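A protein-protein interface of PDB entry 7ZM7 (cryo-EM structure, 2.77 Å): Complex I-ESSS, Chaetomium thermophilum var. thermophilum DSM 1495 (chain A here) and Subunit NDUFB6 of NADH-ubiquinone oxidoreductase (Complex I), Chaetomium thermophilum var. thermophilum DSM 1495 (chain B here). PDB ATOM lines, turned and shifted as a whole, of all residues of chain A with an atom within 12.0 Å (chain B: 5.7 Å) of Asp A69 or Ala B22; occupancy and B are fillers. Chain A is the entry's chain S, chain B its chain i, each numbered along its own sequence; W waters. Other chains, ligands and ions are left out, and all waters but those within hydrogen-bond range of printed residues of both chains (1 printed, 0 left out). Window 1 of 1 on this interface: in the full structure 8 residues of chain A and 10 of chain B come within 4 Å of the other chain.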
ATOM      1  N   GLN A  67       0.254   3.743   9.558  1.00  0.00           N
ATOM      2  CA  GLN A  67      -0.870   3.024   8.973  1.00  0.00           C
ATOM      3  C   GLN A  67      -2.117   3.134   9.830  1.00  0.00           C
ATOM      4  O   GLN A  67      -2.114   2.812  11.009  1.00  0.00           O
ATOM      5  CB  GLN A  67      -0.514   1.554   8.758  1.00  0.00           C
ATOM      6  CG  GLN A  67       0.623   1.341   7.784  1.00  0.00           C
ATOM      7  CD  GLN A  67       0.753  -0.105   7.359  1.00  0.00           C
ATOM      8  OE1 GLN A  67       0.011  -0.968   7.826  1.00  0.00           O
ATOM      9  NE2 GLN A  67       1.696  -0.376   6.466  1.00  0.00           N
ATOM     10  N   TYR A  68      -3.196   3.558   9.192  1.00  0.00           N
ATOM     11  CA  TYR A  68      -4.464   3.839   9.892  1.00  0.00           C
ATOM     12  C   TYR A  68      -5.126   2.606  10.495  1.00  0.00           C
ATOM     13  O   TYR A  68      -5.152   1.549   9.849  1.00  0.00           O
ATOM     14  CB  TYR A  68      -5.351   4.584   8.900  1.00  0.00           C
ATOM     15  CG  TYR A  68      -4.775   5.907   8.475  1.00  0.00           C
ATOM     16  CD1 TYR A  68      -4.360   6.833   9.414  1.00  0.00           C
ATOM     17  CD2 TYR A  68      -4.625   6.228   7.139  1.00  0.00           C
ATOM     18  CE1 TYR A  68      -3.817   8.048   9.036  1.00  0.00           C
ATOM     19  CE2 TYR A  68      -4.091   7.442   6.743  1.00  0.00           C
ATOM     20  CZ  TYR A  68      -3.687   8.355   7.695  1.00  0.00           C
ATOM     21  OH  TYR A  68      -3.152   9.549   7.319  1.00  0.00           O
ATOM     22  N   ASP A  69      -5.661   2.756  11.697  1.00  0.00           N
ATOM     23  CA  ASP A  69      -6.359   1.668  12.408  1.00  0.00           C
ATOM     24  C   ASP A  69      -7.797   1.520  11.899  1.00  0.00           C
ATOM     25  O   ASP A  69      -8.310   2.448  11.271  1.00  0.00           O
ATOM     26  CB  ASP A  69      -6.363   1.998  13.892  1.00  0.00           C
ATOM     27  CG  ASP A  69      -5.071   1.619  14.589  1.00  0.00           C
ATOM     28  OD1 ASP A  69      -4.318   0.814  14.007  1.00  0.00           O
ATOM     29  OD2 ASP A  69      -4.828   2.129  15.702  1.00  0.00           O
ATOM     30  N   PRO A  70      -8.476   0.376  12.130  1.00  0.00           N
ATOM     31  CA  PRO A  70      -9.887   0.230  11.758  1.00  0.00           C
ATOM     32  C   PRO A  70     -10.863   1.103  12.563  1.00  0.00           C
ATOM     33  O   PRO A  70     -10.564   1.441  13.703  1.00  0.00           O
ATOM     34  CB  PRO A  70     -10.124  -1.204  12.205  1.00  0.00           C
ATOM     35  CG  PRO A  70      -9.147  -1.441  13.311  1.00  0.00           C
ATOM     36  CD  PRO A  70      -7.903  -0.822  12.736  1.00  0.00           C
ATOM     37  N   PRO A  71     -12.051   1.463  12.043  1.00  0.00           N
ATOM     38  CA  PRO A  71     -12.936   2.373  12.762  1.00  0.00           C
ATOM     39  C   PRO A  71     -13.627   1.532  13.824  1.00  0.00           C
ATOM     40  O   PRO A  71     -13.738   0.349  13.607  1.00  0.00           O
ATOM     41  CB  PRO A  71     -13.894   2.886  11.682  1.00  0.00           C
ATOM     42  CG  PRO A  71     -13.327   2.386  10.371  1.00  0.00           C
ATOM     43  CD  PRO A  71     -12.553   1.132  10.713  1.00  0.00           C
ATOM     44  N   THR A  72     -14.048   2.128  14.941  1.00  0.00           N
ATOM     45  CA  THR A  72     -14.533   1.266  16.002  1.00  0.00           C
ATOM     46  C   THR A  72     -15.579   2.027  16.801  1.00  0.00           C
ATOM     47  O   THR A  72     -16.042   3.093  16.393  1.00  0.00           O
ATOM     48  CB  THR A  72     -13.365   0.774  16.866  1.00  0.00           C
ATOM     49  OG1 THR A  72     -13.812  -0.267  17.743  1.00  0.00           O
ATOM     50  CG2 THR A  72     -12.768   1.912  17.681  1.00  0.00           C
ATOM     51  N   GLY A  73     -15.956   1.469  17.946  1.00  0.00           N
ATOM     52  CA  GLY A  73     -16.847   2.215  18.846  1.00  0.00           C
ATOM     53  C   GLY A  73     -18.157   1.528  19.093  1.00  0.00           C
ATOM     54  O   GLY A  73     -18.660   0.869  18.182  1.00  0.00           O
ATOM     55  N   TRP A  74     -18.689   1.675  20.297  1.00  0.00           N
ATOM     56  CA  TRP A  74     -20.051   1.157  20.530  1.00  0.00           C
ATOM     57  C   TRP A  74     -20.992   2.351  20.430  1.00  0.00           C
ATOM     58  O   TRP A  74     -21.023   3.146  21.377  1.00  0.00           O
ATOM     59  CB  TRP A  74     -20.146   0.472  21.887  1.00  0.00           C
ATOM     60  CG  TRP A  74     -19.134  -0.612  22.081  1.00  0.00           C
ATOM     61  CD1 TRP A  74     -18.393  -1.230  21.117  1.00  0.00           C
ATOM     62  CD2 TRP A  74     -18.744  -1.206  23.329  1.00  0.00           C
ATOM     63  NE1 TRP A  74     -17.566  -2.161  21.679  1.00  0.00           N
ATOM     64  CE2 TRP A  74     -17.763  -2.173  23.033  1.00  0.00           C
ATOM     65  CE3 TRP A  74     -19.130  -1.016  24.659  1.00  0.00           C
ATOM     66  CZ2 TRP A  74     -17.164  -2.946  24.023  1.00  0.00           C
ATOM     67  CZ3 TRP A  74     -18.536  -1.781  25.636  1.00  0.00           C
ATOM     68  CH2 TRP A  74     -17.570  -2.732  25.318  1.00  0.00           C
ATOM     69  N   LYS B   6       2.075   4.959  17.704  1.00  0.00           N
ATOM     70  CA  LYS B   6       0.684   5.361  17.810  1.00  0.00           C
ATOM     71  C   LYS B   6       0.196   5.241  19.246  1.00  0.00           C
ATOM     72  O   LYS B   6       0.514   4.281  19.953  1.00  0.00           O
ATOM     73  CB  LYS B   6      -0.151   4.500  16.873  1.00  0.00           C
ATOM     74  CG  LYS B   6       0.139   4.822  15.429  1.00  0.00           C
ATOM     75  CD  LYS B   6      -0.544   3.884  14.485  1.00  0.00           C
ATOM     76  CE  LYS B   6      -2.003   4.061  14.429  1.00  0.00           C
ATOM     77  NZ  LYS B   6      -2.538   3.167  13.390  1.00  0.00           N
ATOM     78  N   TYR B   9      -5.320   3.684  22.817  1.00  0.00           N
ATOM     79  CA  TYR B   9      -6.611   4.320  23.020  1.00  0.00           C
ATOM     80  C   TYR B   9      -7.635   3.247  23.330  1.00  0.00           C
ATOM     81  O   TYR B   9      -7.411   2.070  23.038  1.00  0.00           O
ATOM     82  CB  TYR B   9      -7.049   5.136  21.798  1.00  0.00           C
ATOM     83  CG  TYR B   9      -7.124   4.372  20.514  1.00  0.00           C
ATOM     84  CD1 TYR B   9      -5.983   4.044  19.807  1.00  0.00           C
ATOM     85  CD2 TYR B   9      -8.345   3.983  20.004  1.00  0.00           C
ATOM     86  CE1 TYR B   9      -6.059   3.352  18.630  1.00  0.00           C
ATOM     87  CE2 TYR B   9      -8.431   3.283  18.835  1.00  0.00           C
ATOM     88  CZ  TYR B   9      -7.290   2.971  18.150  1.00  0.00           C
ATOM     89  OH  TYR B   9      -7.392   2.274  16.976  1.00  0.00           O
ATOM     90  N   LYS B  11     -10.895   1.160  22.607  1.00  0.00           N
ATOM     91  CA  LYS B  11     -11.559   0.788  21.369  1.00  0.00           C
ATOM     92  C   LYS B  11     -13.079   0.798  21.469  1.00  0.00           C
ATOM     93  O   LYS B  11     -13.748   0.535  20.472  1.00  0.00           O
ATOM     94  CB  LYS B  11     -11.077  -0.583  20.925  1.00  0.00           C
ATOM     95  CG  LYS B  11      -9.580  -0.798  21.091  1.00  0.00           C
ATOM     96  CD  LYS B  11      -8.757   0.045  20.143  1.00  0.00           C
ATOM     97  CE  LYS B  11      -7.462  -0.667  19.772  1.00  0.00           C
ATOM     98  NZ  LYS B  11      -6.304   0.254  19.520  1.00  0.00           N
ATOM     99  N   ALA B  17     -16.130  11.796  14.167  1.00  0.00           N
ATOM    100  CA  ALA B  17     -14.999  12.220  13.362  1.00  0.00           C
ATOM    101  C   ALA B  17     -13.901  11.168  13.315  1.00  0.00           C
ATOM    102  O   ALA B  17     -12.764  11.478  12.970  1.00  0.00           O
ATOM    103  CB  ALA B  17     -14.457  13.551  13.872  1.00  0.00           C
ATOM    104  N   GLY B  18     -14.226   9.930  13.647  1.00  0.00           N
ATOM    105  CA  GLY B  18     -13.287   8.842  13.536  1.00  0.00           C
ATOM    106  C   GLY B  18     -12.680   8.418  14.851  1.00  0.00           C
ATOM    107  O   GLY B  18     -12.566   7.229  15.136  1.00  0.00           O
ATOM    108  N   GLY B  19     -12.306   9.368  15.674  1.00  0.00           N
ATOM    109  CA  GLY B  19     -11.558   9.057  16.876  1.00  0.00           C
ATOM    110  C   GLY B  19     -10.079   8.999  16.570  1.00  0.00           C
ATOM    111  O   GLY B  19      -9.531   9.921  15.975  1.00  0.00           O
ATOM    112  N   TRP B  20      -9.442   7.897  16.948  1.00  0.00           N
ATOM    113  CA  TRP B  20      -8.004   7.738  16.806  1.00  0.00           C
ATOM    114  C   TRP B  20      -7.691   6.969  15.527  1.00  0.00           C
ATOM    115  O   TRP B  20      -8.142   5.837  15.358  1.00  0.00           O
ATOM    116  CB  TRP B  20      -7.419   7.019  18.016  1.00  0.00           C
ATOM    117  CG  TRP B  20      -7.420   7.768  19.329  1.00  0.00           C
ATOM    118  CD1 TRP B  20      -6.392   8.466  19.855  1.00  0.00           C
ATOM    119  CD2 TRP B  20      -8.485   7.858  20.281  1.00  0.00           C
ATOM    120  NE1 TRP B  20      -6.740   8.995  21.063  1.00  0.00           N
ATOM    121  CE2 TRP B  20      -8.024   8.631  21.347  1.00  0.00           C
ATOM    122  CE3 TRP B  20      -9.779   7.353  20.337  1.00  0.00           C
ATOM    123  CZ2 TRP B  20      -8.809   8.917  22.448  1.00  0.00           C
ATOM    124  CZ3 TRP B  20     -10.555   7.644  21.429  1.00  0.00           C
ATOM    125  CH2 TRP B  20     -10.066   8.408  22.473  1.00  0.00           C
ATOM    126  N   TYR B  21      -6.937   7.599  14.626  1.00  0.00           N
ATOM    127  CA  TYR B  21      -6.283   6.930  13.499  1.00  0.00           C
ATOM    128  C   TYR B  21      -7.275   6.256  12.557  1.00  0.00           C
ATOM    129  O   TYR B  21      -6.913   5.379  11.774  1.00  0.00           O
ATOM    130  CB  TYR B  21      -5.251   5.919  13.996  1.00  0.00           C
ATOM    131  CG  TYR B  21      -4.184   6.529  14.848  1.00  0.00           C
ATOM    132  CD1 TYR B  21      -3.349   7.509  14.332  1.00  0.00           C
ATOM    133  CD2 TYR B  21      -4.004   6.138  16.162  1.00  0.00           C
ATOM    134  CE1 TYR B  21      -2.377   8.075  15.095  1.00  0.00           C
ATOM    135  CE2 TYR B  21      -3.015   6.695  16.930  1.00  0.00           C
ATOM    136  CZ  TYR B  21      -2.211   7.669  16.388  1.00  0.00           C
ATOM    137  OH  TYR B  21      -1.229   8.251  17.133  1.00  0.00           O
ATOM    138  N   ALA B  22      -8.543   6.656  12.659  1.00  0.00           N
ATOM    139  CA  ALA B  22      -9.617   5.928  11.947  1.00  0.00           C
ATOM    140  C   ALA B  22      -9.713   6.173  10.450  1.00  0.00           C
ATOM    141  O   ALA B  22     -10.081   7.285  10.049  1.00  0.00           O
ATOM    142  CB  ALA B  22     -10.932   6.224  12.608  1.00  0.00           C
ATOM    143  N   GLN B  23      -9.400   5.150   9.661  1.00  0.00           N
ATOM    144  CA  GLN B  23      -9.639   5.232   8.207  1.00  0.00           C
ATOM    145  C   GLN B  23     -10.339   3.926   7.867  1.00  0.00           C
ATOM    146  O   GLN B  23      -9.752   2.876   8.154  1.00  0.00           O
ATOM    147  CB  GLN B  23      -8.319   5.341   7.452  1.00  0.00           C
ATOM    148  CG  GLN B  23      -8.466   5.237   5.944  1.00  0.00           C
ATOM    149  CD  GLN B  23      -7.590   6.265   5.277  1.00  0.00           C
ATOM    150  OE1 GLN B  23      -7.431   7.374   5.776  1.00  0.00           O
ATOM    151  NE2 GLN B  23      -7.000   5.897   4.153  1.00  0.00           N
ATOM    152  N   PRO B  24     -11.562   3.917   7.302  1.00  0.00           N
ATOM    153  CA  PRO B  24     -12.173   2.663   6.899  1.00  0.00           C
ATOM    154  C   PRO B  24     -11.516   2.122   5.624  1.00  0.00           C
ATOM    155  O   PRO B  24     -10.765   2.838   5.016  1.00  0.00           O
ATOM    156  CB  PRO B  24     -13.640   3.045   6.648  1.00  0.00           C
ATOM    157  CG  PRO B  24     -13.597   4.515   6.312  1.00  0.00           C
ATOM    158  CD  PRO B  24     -12.425   5.074   7.090  1.00  0.00           C
HETATM  159  O   HOH W   1     -11.806   4.490  15.859  1.00  0.00           O
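The backbone carbonyl oxygen (O) of Asp A69 sits at hydrogen-bond distance from the backbone NH (N) of Gln B23, at 3.3 Å. The side-chain carboxylate (OD2) of Asp A69 lies within hydrogen-bond range of the side-chain hydroxyl (OH) of Tyr B9 (2.9 Å). The backbone carbonyl oxygen (O) of Gln A67 is in hydrogen-bond range of the side-chain amino group (NZ) of Lys B6. OG1 of Thr A72 is in hydrogen-bond range of O of Lys B11, at 2.8 Å. The backbone carbonyl oxygen (O) of Tyr B21 lies within hydrogen-bond range of the backbone NH (N) of Asp A69 (2.9 Å). The side-chain amino group of Lys B6 is in salt-bridge range of the side-chain carboxylate of Asp A69 (3.0 Å). N of Gly A73 is in hydrogen-bond range of O of Lys B11 (3.5 Å).
The side-chain amino group (NZ) of Lys B11 lies close to the side-chain hydroxyl (OH) of Tyr B9 (3.4 Å).
Tyr A68 touches Lys B6. Tyr B21 touches Tyr A68. Tyr A68 touches Gln B23. Asp A69 touches Ala B22. CA of Pro B24 touches CG of Pro A71, 3.7 Å away.
Of chain A, only Asp A69 comes within 4 Å of Ala B22. Lys B6 touches just these residues of chain A: Gln A67, Tyr A68 and Asp A69. Gly B18 touches none of the printed residues of chain A. Gly B19 touches none of the printed residues of chain A. Tyr B21 touches just these residues of chain A: Tyr A68 and Asp A69. Pro B24 touches just one residue of chain A: Pro A71 (3.7 Å). Printed residues of chain A within 4 Å of Tyr B9: Asp A69. Of the printed residues of chain A, Lys B11 touches Thr A72 and Gly A73. Printed residues of chain B within 4 Å of Gln A67: Lys B6 (2.4 Å). Of the printed residues of chain B, Thr A72 touches Lys B11.
Hydrophobic or aromatic side chains of chain A within 4 Å of the printed part of chain B: Tyr A68 and Pro A71. Among the printed residues, 12 pairs touch across the chains.
Water W1 lies within hydrogen-bond range of O of Gly B18 and N of Thr A72.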
